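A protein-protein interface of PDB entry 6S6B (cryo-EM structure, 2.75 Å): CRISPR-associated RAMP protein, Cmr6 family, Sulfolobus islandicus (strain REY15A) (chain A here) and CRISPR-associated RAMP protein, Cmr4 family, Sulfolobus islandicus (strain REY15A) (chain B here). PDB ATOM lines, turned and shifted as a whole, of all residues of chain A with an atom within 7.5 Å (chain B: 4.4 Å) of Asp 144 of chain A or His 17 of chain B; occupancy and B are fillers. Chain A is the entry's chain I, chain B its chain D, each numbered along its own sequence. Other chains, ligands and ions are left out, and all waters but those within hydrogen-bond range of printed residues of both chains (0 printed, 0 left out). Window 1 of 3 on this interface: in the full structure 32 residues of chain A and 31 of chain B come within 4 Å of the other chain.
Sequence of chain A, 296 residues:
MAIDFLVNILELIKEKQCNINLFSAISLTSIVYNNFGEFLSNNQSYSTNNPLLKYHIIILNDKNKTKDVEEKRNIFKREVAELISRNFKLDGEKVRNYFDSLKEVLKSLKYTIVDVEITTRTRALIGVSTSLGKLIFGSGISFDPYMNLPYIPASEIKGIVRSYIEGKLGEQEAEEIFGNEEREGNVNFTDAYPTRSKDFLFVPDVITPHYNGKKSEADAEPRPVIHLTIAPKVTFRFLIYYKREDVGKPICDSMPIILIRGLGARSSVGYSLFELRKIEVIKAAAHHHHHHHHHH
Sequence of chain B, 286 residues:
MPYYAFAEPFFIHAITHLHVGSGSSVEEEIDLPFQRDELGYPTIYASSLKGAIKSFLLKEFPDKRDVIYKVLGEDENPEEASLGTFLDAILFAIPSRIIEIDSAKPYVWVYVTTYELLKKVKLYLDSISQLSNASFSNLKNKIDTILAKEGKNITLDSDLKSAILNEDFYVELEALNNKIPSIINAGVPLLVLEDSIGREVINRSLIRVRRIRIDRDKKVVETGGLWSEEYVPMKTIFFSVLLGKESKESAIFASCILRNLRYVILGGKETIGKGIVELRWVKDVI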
ATOM      1  N   ASN A  21     -39.056  19.378   9.210  1.00  0.00           N
ATOM      2  CA  ASN A  21     -38.030  18.400   8.890  1.00  0.00           C
ATOM      3  C   ASN A  21     -37.384  18.856   7.594  1.00  0.00           C
ATOM      4  O   ASN A  21     -37.961  18.706   6.517  1.00  0.00           O
ATOM      5  CB  ASN A  21     -38.623  17.006   8.771  1.00  0.00           C
ATOM      6  CG  ASN A  21     -37.570  15.937   8.774  1.00  0.00           C
ATOM      7  OD1 ASN A  21     -37.076  15.542   9.825  1.00  0.00           O
ATOM      8  ND2 ASN A  21     -37.207  15.465   7.596  1.00  0.00           N
ATOM      9  N   LEU A  22     -36.188  19.434   7.695  1.00  0.00           N
ATOM     10  CA  LEU A  22     -35.549  19.995   6.512  1.00  0.00           C
ATOM     11  C   LEU A  22     -35.268  18.919   5.480  1.00  0.00           C
ATOM     12  O   LEU A  22     -35.352  19.168   4.273  1.00  0.00           O
ATOM     13  CB  LEU A  22     -34.262  20.716   6.894  1.00  0.00           C
ATOM     14  CG  LEU A  22     -33.495  21.274   5.698  1.00  0.00           C
ATOM     15  CD1 LEU A  22     -34.271  22.413   5.077  1.00  0.00           C
ATOM     16  CD2 LEU A  22     -32.112  21.722   6.097  1.00  0.00           C
ATOM     17  N   PHE A  23     -34.942  17.711   5.934  1.00  0.00           N
ATOM     18  CA  PHE A  23     -34.688  16.622   5.002  1.00  0.00           C
ATOM     19  C   PHE A  23     -35.912  16.347   4.143  1.00  0.00           C
ATOM     20  O   PHE A  23     -35.826  16.312   2.913  1.00  0.00           O
ATOM     21  CB  PHE A  23     -34.276  15.368   5.762  1.00  0.00           C
ATOM     22  CG  PHE A  23     -33.684  14.311   4.890  1.00  0.00           C
ATOM     23  CD1 PHE A  23     -34.487  13.510   4.107  1.00  0.00           C
ATOM     24  CD2 PHE A  23     -32.319  14.122   4.850  1.00  0.00           C
ATOM     25  CE1 PHE A  23     -33.947  12.548   3.304  1.00  0.00           C
ATOM     26  CE2 PHE A  23     -31.772  13.155   4.050  1.00  0.00           C
ATOM     27  CZ  PHE A  23     -32.588  12.367   3.274  1.00  0.00           C
ATOM     28  N   LYS A  94     -30.872  22.130  21.826  1.00  0.00           N
ATOM     29  CA  LYS A  94     -31.136  20.699  21.866  1.00  0.00           C
ATOM     30  C   LYS A  94     -29.876  19.876  21.662  1.00  0.00           C
ATOM     31  O   LYS A  94     -29.837  18.716  22.080  1.00  0.00           O
ATOM     32  CB  LYS A  94     -32.171  20.322  20.813  1.00  0.00           C
ATOM     33  CG  LYS A  94     -31.698  20.538  19.399  1.00  0.00           C
ATOM     34  CD  LYS A  94     -32.737  20.080  18.404  1.00  0.00           C
ATOM     35  CE  LYS A  94     -32.304  20.397  16.987  1.00  0.00           C
ATOM     36  NZ  LYS A  94     -33.372  20.072  16.008  1.00  0.00           N
ATOM     37  N   TYR A  98     -28.185  17.525  24.431  1.00  0.00           N
ATOM     38  CA  TYR A  98     -27.855  16.177  23.988  1.00  0.00           C
ATOM     39  C   TYR A  98     -26.452  15.789  24.422  1.00  0.00           C
ATOM     40  O   TYR A  98     -26.252  14.748  25.054  1.00  0.00           O
ATOM     41  CB  TYR A  98     -27.985  16.077  22.474  1.00  0.00           C
ATOM     42  CG  TYR A  98     -27.372  14.830  21.901  1.00  0.00           C
ATOM     43  CD1 TYR A  98     -28.008  13.606  22.022  1.00  0.00           C
ATOM     44  CD2 TYR A  98     -26.162  14.873  21.235  1.00  0.00           C
ATOM     45  CE1 TYR A  98     -27.453  12.465  21.500  1.00  0.00           C
ATOM     46  CE2 TYR A  98     -25.601  13.734  20.711  1.00  0.00           C
ATOM     47  CZ  TYR A  98     -26.251  12.535  20.847  1.00  0.00           C
ATOM     48  OH  TYR A  98     -25.696  11.398  20.322  1.00  0.00           O
ATOM     49  N   LEU A 132     -29.103  15.288   0.306  1.00  0.00           N
ATOM     50  CA  LEU A 132     -29.835  16.407   0.894  1.00  0.00           C
ATOM     51  C   LEU A 132     -29.738  17.549  -0.113  1.00  0.00           C
ATOM     52  O   LEU A 132     -28.697  18.202  -0.208  1.00  0.00           O
ATOM     53  CB  LEU A 132     -29.275  16.807   2.246  1.00  0.00           C
ATOM     54  CG  LEU A 132     -29.919  18.079   2.805  1.00  0.00           C
ATOM     55  CD1 LEU A 132     -31.305  17.792   3.333  1.00  0.00           C
ATOM     56  CD2 LEU A 132     -29.061  18.723   3.871  1.00  0.00           C
ATOM     57  N   ILE A 141     -25.371  17.441   1.784  1.00  0.00           N
ATOM     58  CA  ILE A 141     -24.671  17.692   3.036  1.00  0.00           C
ATOM     59  C   ILE A 141     -25.043  16.576   3.995  1.00  0.00           C
ATOM     60  O   ILE A 141     -26.195  16.136   4.025  1.00  0.00           O
ATOM     61  CB  ILE A 141     -25.021  19.070   3.641  1.00  0.00           C
ATOM     62  CG1 ILE A 141     -24.536  20.208   2.749  1.00  0.00           C
ATOM     63  CG2 ILE A 141     -24.418  19.225   5.013  1.00  0.00           C
ATOM     64  CD1 ILE A 141     -25.565  20.693   1.768  1.00  0.00           C
ATOM     65  N   SER A 142     -24.064  16.095   4.758  1.00  0.00           N
ATOM     66  CA  SER A 142     -24.363  15.102   5.777  1.00  0.00           C
ATOM     67  C   SER A 142     -25.382  15.681   6.738  1.00  0.00           C
ATOM     68  O   SER A 142     -25.071  16.595   7.503  1.00  0.00           O
ATOM     69  CB  SER A 142     -23.105  14.681   6.529  1.00  0.00           C
ATOM     70  OG  SER A 142     -22.216  13.980   5.692  1.00  0.00           O
ATOM     71  N   PHE A 143     -26.598  15.152   6.710  1.00  0.00           N
ATOM     72  CA  PHE A 143     -27.706  15.714   7.462  1.00  0.00           C
ATOM     73  C   PHE A 143     -28.332  14.624   8.307  1.00  0.00           C
ATOM     74  O   PHE A 143     -28.665  13.553   7.794  1.00  0.00           O
ATOM     75  CB  PHE A 143     -28.748  16.319   6.527  1.00  0.00           C
ATOM     76  CG  PHE A 143     -29.681  17.270   7.199  1.00  0.00           C
ATOM     77  CD1 PHE A 143     -29.282  18.557   7.493  1.00  0.00           C
ATOM     78  CD2 PHE A 143     -30.960  16.879   7.538  1.00  0.00           C
ATOM     79  CE1 PHE A 143     -30.138  19.431   8.113  1.00  0.00           C
ATOM     80  CE2 PHE A 143     -31.816  17.751   8.155  1.00  0.00           C
ATOM     81  CZ  PHE A 143     -31.403  19.028   8.443  1.00  0.00           C
ATOM     82  N   ASP A 144     -28.487  14.897   9.587  1.00  0.00           N
ATOM     83  CA  ASP A 144     -29.168  13.985  10.489  1.00  0.00           C
ATOM     84  C   ASP A 144     -30.650  14.326  10.500  1.00  0.00           C
ATOM     85  O   ASP A 144     -31.053  15.305  11.136  1.00  0.00           O
ATOM     86  CB  ASP A 144     -28.579  14.085  11.892  1.00  0.00           C
ATOM     87  CG  ASP A 144     -29.037  12.974  12.785  1.00  0.00           C
ATOM     88  OD1 ASP A 144     -29.847  12.146  12.327  1.00  0.00           O
ATOM     89  OD2 ASP A 144     -28.585  12.920  13.944  1.00  0.00           O
ATOM     90  N   PRO A 145     -31.495  13.550   9.817  1.00  0.00           N
ATOM     91  CA  PRO A 145     -32.898  13.948   9.667  1.00  0.00           C
ATOM     92  C   PRO A 145     -33.702  13.885  10.950  1.00  0.00           C
ATOM     93  O   PRO A 145     -34.868  14.287  10.941  1.00  0.00           O
ATOM     94  CB  PRO A 145     -33.427  12.955   8.631  1.00  0.00           C
ATOM     95  CG  PRO A 145     -32.575  11.779   8.776  1.00  0.00           C
ATOM     96  CD  PRO A 145     -31.221  12.252   9.185  1.00  0.00           C
ATOM     97  N   TYR A 146     -33.128  13.415  12.052  1.00  0.00           N
ATOM     98  CA  TYR A 146     -33.842  13.358  13.317  1.00  0.00           C
ATOM     99  C   TYR A 146     -33.348  14.365  14.335  1.00  0.00           C
ATOM    100  O   TYR A 146     -34.138  14.832  15.153  1.00  0.00           O
ATOM    101  CB  TYR A 146     -33.765  11.945  13.896  1.00  0.00           C
ATOM    102  CG  TYR A 146     -34.331  10.946  12.928  1.00  0.00           C
ATOM    103  CD1 TYR A 146     -35.693  10.853  12.724  1.00  0.00           C
ATOM    104  CD2 TYR A 146     -33.503  10.135  12.178  1.00  0.00           C
ATOM    105  CE1 TYR A 146     -36.213   9.965  11.826  1.00  0.00           C
ATOM    106  CE2 TYR A 146     -34.019   9.245  11.275  1.00  0.00           C
ATOM    107  CZ  TYR A 146     -35.374   9.163  11.107  1.00  0.00           C
ATOM    108  OH  TYR A 146     -35.893   8.273  10.208  1.00  0.00           O
ATOM    109  N   MET A 147     -32.067  14.713  14.306  1.00  0.00           N
ATOM    110  CA  MET A 147     -31.628  15.944  14.939  1.00  0.00           C
ATOM    111  C   MET A 147     -31.929  17.159  14.081  1.00  0.00           C
ATOM    112  O   MET A 147     -31.832  18.283  14.579  1.00  0.00           O
ATOM    113  CB  MET A 147     -30.134  15.887  15.239  1.00  0.00           C
ATOM    114  CG  MET A 147     -29.783  14.983  16.395  1.00  0.00           C
ATOM    115  SD  MET A 147     -30.128  15.741  17.986  1.00  0.00           S
ATOM    116  CE  MET A 147     -28.697  16.788  18.151  1.00  0.00           C
ATOM    117  N   ASN A 148     -32.297  16.955  12.817  1.00  0.00           N
ATOM    118  CA  ASN A 148     -32.626  18.037  11.895  1.00  0.00           C
ATOM    119  C   ASN A 148     -31.478  19.033  11.800  1.00  0.00           C
ATOM    120  O   ASN A 148     -31.664  20.242  11.928  1.00  0.00           O
ATOM    121  CB  ASN A 148     -33.920  18.735  12.304  1.00  0.00           C
ATOM    122  CG  ASN A 148     -34.703  19.241  11.121  1.00  0.00           C
ATOM    123  OD1 ASN A 148     -34.660  18.656  10.043  1.00  0.00           O
ATOM    124  ND2 ASN A 148     -35.429  20.329  11.314  1.00  0.00           N
ATOM    125  N   LEU A 149     -30.280  18.512  11.567  1.00  0.00           N
ATOM    126  CA  LEU A 149     -29.077  19.325  11.577  1.00  0.00           C
ATOM    127  C   LEU A 149     -28.040  18.681  10.681  1.00  0.00           C
ATOM    128  O   LEU A 149     -28.008  17.452  10.562  1.00  0.00           O
ATOM    129  CB  LEU A 149     -28.513  19.465  12.993  1.00  0.00           C
ATOM    130  CG  LEU A 149     -29.154  20.523  13.875  1.00  0.00           C
ATOM    131  CD1 LEU A 149     -28.385  20.632  15.148  1.00  0.00           C
ATOM    132  CD2 LEU A 149     -29.171  21.846  13.159  1.00  0.00           C
ATOM    133  N   PRO A 150     -27.182  19.467  10.045  1.00  0.00           N
ATOM    134  CA  PRO A 150     -26.004  18.891   9.402  1.00  0.00           C
ATOM    135  C   PRO A 150     -25.086  18.306  10.455  1.00  0.00           C
ATOM    136  O   PRO A 150     -25.183  18.619  11.639  1.00  0.00           O
ATOM    137  CB  PRO A 150     -25.361  20.089   8.705  1.00  0.00           C
ATOM    138  CG  PRO A 150     -25.775  21.238   9.529  1.00  0.00           C
ATOM    139  CD  PRO A 150     -27.175  20.935   9.967  1.00  0.00           C
ATOM    140  N   TYR A 151     -24.185  17.437  10.017  1.00  0.00           N
ATOM    141  CA  TYR A 151     -23.272  16.839  10.974  1.00  0.00           C
ATOM    142  C   TYR A 151     -22.069  16.278  10.242  1.00  0.00           C
ATOM    143  O   TYR A 151     -22.082  16.114   9.024  1.00  0.00           O
ATOM    144  CB  TYR A 151     -23.963  15.753  11.800  1.00  0.00           C
ATOM    145  CG  TYR A 151     -24.087  14.433  11.098  1.00  0.00           C
ATOM    146  CD1 TYR A 151     -24.935  14.277  10.025  1.00  0.00           C
ATOM    147  CD2 TYR A 151     -23.358  13.341  11.517  1.00  0.00           C
ATOM    148  CE1 TYR A 151     -25.049  13.076   9.386  1.00  0.00           C
ATOM    149  CE2 TYR A 151     -23.465  12.137  10.882  1.00  0.00           C
ATOM    150  CZ  TYR A 151     -24.312  12.010   9.818  1.00  0.00           C
ATOM    151  OH  TYR A 151     -24.423  10.805   9.178  1.00  0.00           O
ATOM    152  N   ASP A 191     -20.470  11.671  16.256  1.00  0.00           N
ATOM    153  CA  ASP A 191     -20.754  12.641  15.215  1.00  0.00           C
ATOM    154  C   ASP A 191     -20.598  14.052  15.766  1.00  0.00           C
ATOM    155  O   ASP A 191     -20.722  14.296  16.966  1.00  0.00           O
ATOM    156  CB  ASP A 191     -22.165  12.457  14.668  1.00  0.00           C
ATOM    157  CG  ASP A 191     -22.530  11.007  14.466  1.00  0.00           C
ATOM    158  OD1 ASP A 191     -21.768  10.286  13.791  1.00  0.00           O
ATOM    159  OD2 ASP A 191     -23.585  10.584  14.980  1.00  0.00           O
ATOM    160  N   TYR A 193     -21.998  17.782  15.791  1.00  0.00           N
ATOM    161  CA  TYR A 193     -23.195  18.538  15.502  1.00  0.00           C
ATOM    162  C   TYR A 193     -22.956  20.020  15.742  1.00  0.00           C
ATOM    163  O   TYR A 193     -22.172  20.394  16.616  1.00  0.00           O
ATOM    164  CB  TYR A 193     -24.364  18.067  16.369  1.00  0.00           C
ATOM    165  CG  TYR A 193     -24.854  16.691  16.017  1.00  0.00           C
ATOM    166  CD1 TYR A 193     -25.629  16.482  14.896  1.00  0.00           C
ATOM    167  CD2 TYR A 193     -24.534  15.601  16.801  1.00  0.00           C
ATOM    168  CE1 TYR A 193     -26.074  15.232  14.569  1.00  0.00           C
ATOM    169  CE2 TYR A 193     -24.974  14.347  16.482  1.00  0.00           C
ATOM    170  CZ  TYR A 193     -25.744  14.168  15.364  1.00  0.00           C
ATOM    171  OH  TYR A 193     -26.190  12.911  15.038  1.00  0.00           O
ATOM    172  N   THR B  16     -27.580   6.865  21.255  1.00  0.00           N
ATOM    173  CA  THR B  16     -27.023   7.201  19.959  1.00  0.00           C
ATOM    174  C   THR B  16     -27.696   6.334  18.902  1.00  0.00           C
ATOM    175  O   THR B  16     -28.655   5.616  19.182  1.00  0.00           O
ATOM    176  CB  THR B  16     -25.515   7.003  19.971  1.00  0.00           C
ATOM    177  OG1 THR B  16     -25.227   5.629  20.244  1.00  0.00           O
ATOM    178  CG2 THR B  16     -24.885   7.849  21.049  1.00  0.00           C
ATOM    179  N   HIS B  17     -27.204   6.386  17.674  1.00  0.00           N
ATOM    180  CA  HIS B  17     -27.654   5.437  16.673  1.00  0.00           C
ATOM    181  C   HIS B  17     -27.158   4.044  17.023  1.00  0.00           C
ATOM    182  O   HIS B  17     -26.118   3.874  17.659  1.00  0.00           O
ATOM    183  CB  HIS B  17     -27.152   5.834  15.293  1.00  0.00           C
ATOM    184  CG  HIS B  17     -27.670   7.152  14.820  1.00  0.00           C
ATOM    185  ND1 HIS B  17     -27.119   7.825  13.755  1.00  0.00           N
ATOM    186  CD2 HIS B  17     -28.694   7.915  15.259  1.00  0.00           C
ATOM    187  CE1 HIS B  17     -27.778   8.951  13.561  1.00  0.00           C
ATOM    188  NE2 HIS B  17     -28.742   9.029  14.459  1.00  0.00           N
ATOM    189  N   LEU B  18     -27.918   3.040  16.613  1.00  0.00           N
ATOM    190  CA  LEU B  18     -27.570   1.652  16.860  1.00  0.00           C
ATOM    191  C   LEU B  18     -27.265   0.966  15.545  1.00  0.00           C
ATOM    192  O   LEU B  18     -27.913   1.233  14.535  1.00  0.00           O
ATOM    193  CB  LEU B  18     -28.700   0.895  17.544  1.00  0.00           C
ATOM    194  CG  LEU B  18     -29.065   1.191  18.987  1.00  0.00           C
ATOM    195  CD1 LEU B  18     -30.270   0.372  19.356  1.00  0.00           C
ATOM    196  CD2 LEU B  18     -27.914   0.860  19.888  1.00  0.00           C
ATOM    197  N   HIS B  19     -26.286   0.072  15.566  1.00  0.00           N
ATOM    198  CA  HIS B  19     -26.109  -0.888  14.485  1.00  0.00           C
ATOM    199  C   HIS B  19     -25.980  -2.268  15.101  1.00  0.00           C
ATOM    200  O   HIS B  19     -24.987  -2.563  15.770  1.00  0.00           O
ATOM    201  CB  HIS B  19     -24.898  -0.571  13.622  1.00  0.00           C
ATOM    202  CG  HIS B  19     -24.748  -1.494  12.458  1.00  0.00           C
ATOM    203  ND1 HIS B  19     -25.558  -1.424  11.347  1.00  0.00           N
ATOM    204  CD2 HIS B  19     -23.897  -2.522  12.241  1.00  0.00           C
ATOM    205  CE1 HIS B  19     -25.204  -2.363  10.490  1.00  0.00           C
ATOM    206  NE2 HIS B  19     -24.200  -3.044  11.008  1.00  0.00           N
ATOM    207  N   ILE B 207     -31.787   4.875   9.282  1.00  0.00           N
ATOM    208  CA  ILE B 207     -30.716   5.671   8.705  1.00  0.00           C
ATOM    209  C   ILE B 207     -29.786   4.754   7.929  1.00  0.00           C
ATOM    210  O   ILE B 207     -29.400   3.686   8.413  1.00  0.00           O
ATOM    211  CB  ILE B 207     -29.962   6.435   9.797  1.00  0.00           C
ATOM    212  CG1 ILE B 207     -30.898   7.433  10.466  1.00  0.00           C
ATOM    213  CG2 ILE B 207     -28.769   7.141   9.216  1.00  0.00           C
ATOM    214  CD1 ILE B 207     -30.489   7.794  11.854  1.00  0.00           C
ATOM    215  N   TYR B 231     -28.359   2.098  10.259  1.00  0.00           N
ATOM    216  CA  TYR B 231     -28.511   2.382  11.671  1.00  0.00           C
ATOM    217  C   TYR B 231     -29.981   2.576  11.986  1.00  0.00           C
ATOM    218  O   TYR B 231     -30.792   2.866  11.107  1.00  0.00           O
ATOM    219  CB  TYR B 231     -27.728   3.624  12.082  1.00  0.00           C
ATOM    220  CG  TYR B 231     -26.327   3.636  11.554  1.00  0.00           C
ATOM    221  CD1 TYR B 231     -25.393   2.724  12.004  1.00  0.00           C
ATOM    222  CD2 TYR B 231     -25.942   4.550  10.597  1.00  0.00           C
ATOM    223  CE1 TYR B 231     -24.116   2.726  11.518  1.00  0.00           C
ATOM    224  CE2 TYR B 231     -24.669   4.560  10.106  1.00  0.00           C
ATOM    225  CZ  TYR B 231     -23.758   3.649  10.570  1.00  0.00           C
ATOM    226  OH  TYR B 231     -22.479   3.665  10.078  1.00  0.00           O
ATOM    227  N   VAL B 232     -30.319   2.406  13.254  1.00  0.00           N
ATOM    228  CA  VAL B 232     -31.665   2.716  13.709  1.00  0.00           C
ATOM    229  C   VAL B 232     -31.530   4.056  14.421  1.00  0.00           C
ATOM    230  O   VAL B 232     -30.530   4.283  15.116  1.00  0.00           O
ATOM    231  CB  VAL B 232     -32.233   1.592  14.593  1.00  0.00           C
ATOM    232  CG1 VAL B 232     -31.721   1.673  16.005  1.00  0.00           C
ATOM    233  CG2 VAL B 232     -33.731   1.551  14.537  1.00  0.00           C
ATOM    234  N   PRO B 233     -32.456   4.990  14.229  1.00  0.00           N
ATOM    235  CA  PRO B 233     -32.256   6.355  14.726  1.00  0.00           C
ATOM    236  C   PRO B 233     -32.055   6.409  16.231  1.00  0.00           C
ATOM    237  O   PRO B 233     -32.250   5.438  16.957  1.00  0.00           O
ATOM    238  CB  PRO B 233     -33.547   7.060  14.319  1.00  0.00           C
ATOM    239  CG  PRO B 233     -34.028   6.303  13.159  1.00  0.00           C
ATOM    240  CD  PRO B 233     -33.645   4.888  13.372  1.00  0.00           C
ATOM    241  N   MET B 234     -31.628   7.577  16.697  1.00  0.00           N
ATOM    242  CA  MET B 234     -31.627   7.835  18.127  1.00  0.00           C
ATOM    243  C   MET B 234     -33.047   7.763  18.661  1.00  0.00           C
ATOM    244  O   MET B 234     -34.013   8.040  17.950  1.00  0.00           O
ATOM    245  CB  MET B 234     -31.051   9.214  18.438  1.00  0.00           C
ATOM    246  CG  MET B 234     -29.577   9.371  18.200  1.00  0.00           C
ATOM    247  SD  MET B 234     -29.158  11.077  17.830  1.00  0.00           S
ATOM    248  CE  MET B 234     -27.412  10.918  17.480  1.00  0.00           C
ATOM    249  N   LYS B 274     -21.685   4.515  17.711  1.00  0.00           N
ATOM    250  CA  LYS B 274     -22.930   3.776  17.735  1.00  0.00           C
ATOM    251  C   LYS B 274     -22.960   2.845  18.937  1.00  0.00           C
ATOM    252  O   LYS B 274     -21.931   2.521  19.529  1.00  0.00           O
ATOM    253  CB  LYS B 274     -23.100   2.975  16.451  1.00  0.00           C
ATOM    254  CG  LYS B 274     -22.772   3.749  15.201  1.00  0.00           C
ATOM    255  CD  LYS B 274     -23.759   4.853  14.979  1.00  0.00           C
ATOM    256  CE  LYS B 274     -23.419   5.644  13.748  1.00  0.00           C
ATOM    257  NZ  LYS B 274     -22.261   6.516  14.010  1.00  0.00           N
ATOM    258  N   GLY B 275     -24.160   2.427  19.308  1.00  0.00           N
ATOM    259  CA  GLY B 275     -24.338   1.329  20.219  1.00  0.00           C
ATOM    260  C   GLY B 275     -24.764   1.697  21.622  1.00  0.00           C
ATOM    261  O   GLY B 275     -25.296   0.838  22.325  1.00  0.00           O
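Of chain B, only His 17 (3.9 Å) comes within 4 Å of Asp 144 of chain A.
Printed residues of chain A within 4 Å of Lys 274 of chain B: Asp 191 (3.8 Å).
Of the printed residues of chain A, Pro 233 of chain B touches Tyr 146.
Of the printed residues of chain A, Ile 207 of chain B touches Tyr 146.
Printed residues of chain B within 4 Å of Tyr 146 of chain A: Ile 207 and Pro 233.
Of the printed residues of chain B, Tyr 193 of chain A touches Met 234.
The nearest residue of chain A that does not touch His 17 of chain B is Tyr 193 of chain A (4.5 Å).
N of Gly 275 of chain B lies within hydrogen-bond range of O of His 17 of chain B (2.9 Å).
O of Ile 207 of chain B lies within hydrogen-bond range of N of Tyr 231 of chain B (2.6 Å).
The backbone carbonyl oxygen of Leu 149 of chain A sits at hydrogen-bond distance from the backbone NH of Asp 144 of chain A (2.8 Å).
OD2 of Asp 144 of chain A lies within hydrogen-bond range of OH of Tyr 193 of chain A, at 2.6 Å.
The side-chain hydroxyl of Tyr 193 of chain A is in hydrogen-bond range of the side-chain carboxylate of Asp 191 of chain A, at 3.5 Å.
Among the printed residues, merely in contact across the chains: Tyr 98 of chain A with Thr 16 of chain B (3.7 Å), Tyr 98 of chain A with Met 234 of chain B (3.4 Å), Asp 144 of chain A with His 17 of chain B (3.9 Å), Tyr 146 of chain A with Ile 207 of chain B (3.7 Å), Tyr 146 of chain A with Pro 233 of chain B (3.5 Å) and Tyr 193 of chain A with Met 234 of chain B (3.4 Å).
The side-chain carboxylate (OD1) of Asp 191 of chain A is in salt-bridge range of the side-chain amino group (NZ) of Lys 274 of chain B.
Of the 19 printed residues of chain A, 5 touch a printed residue of chain B.
Printed residues of chain A that touch a printed residue of chain B: Tyr 98, Asp 144, Tyr 146, Asp 191 and Tyr 193.
Hydrophobic or aromatic side chains of chain A that line the printed part of chain B: Tyr 98, Tyr 146 and Tyr 193.
Among the printed residues, 7 pairs touch across the chains.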
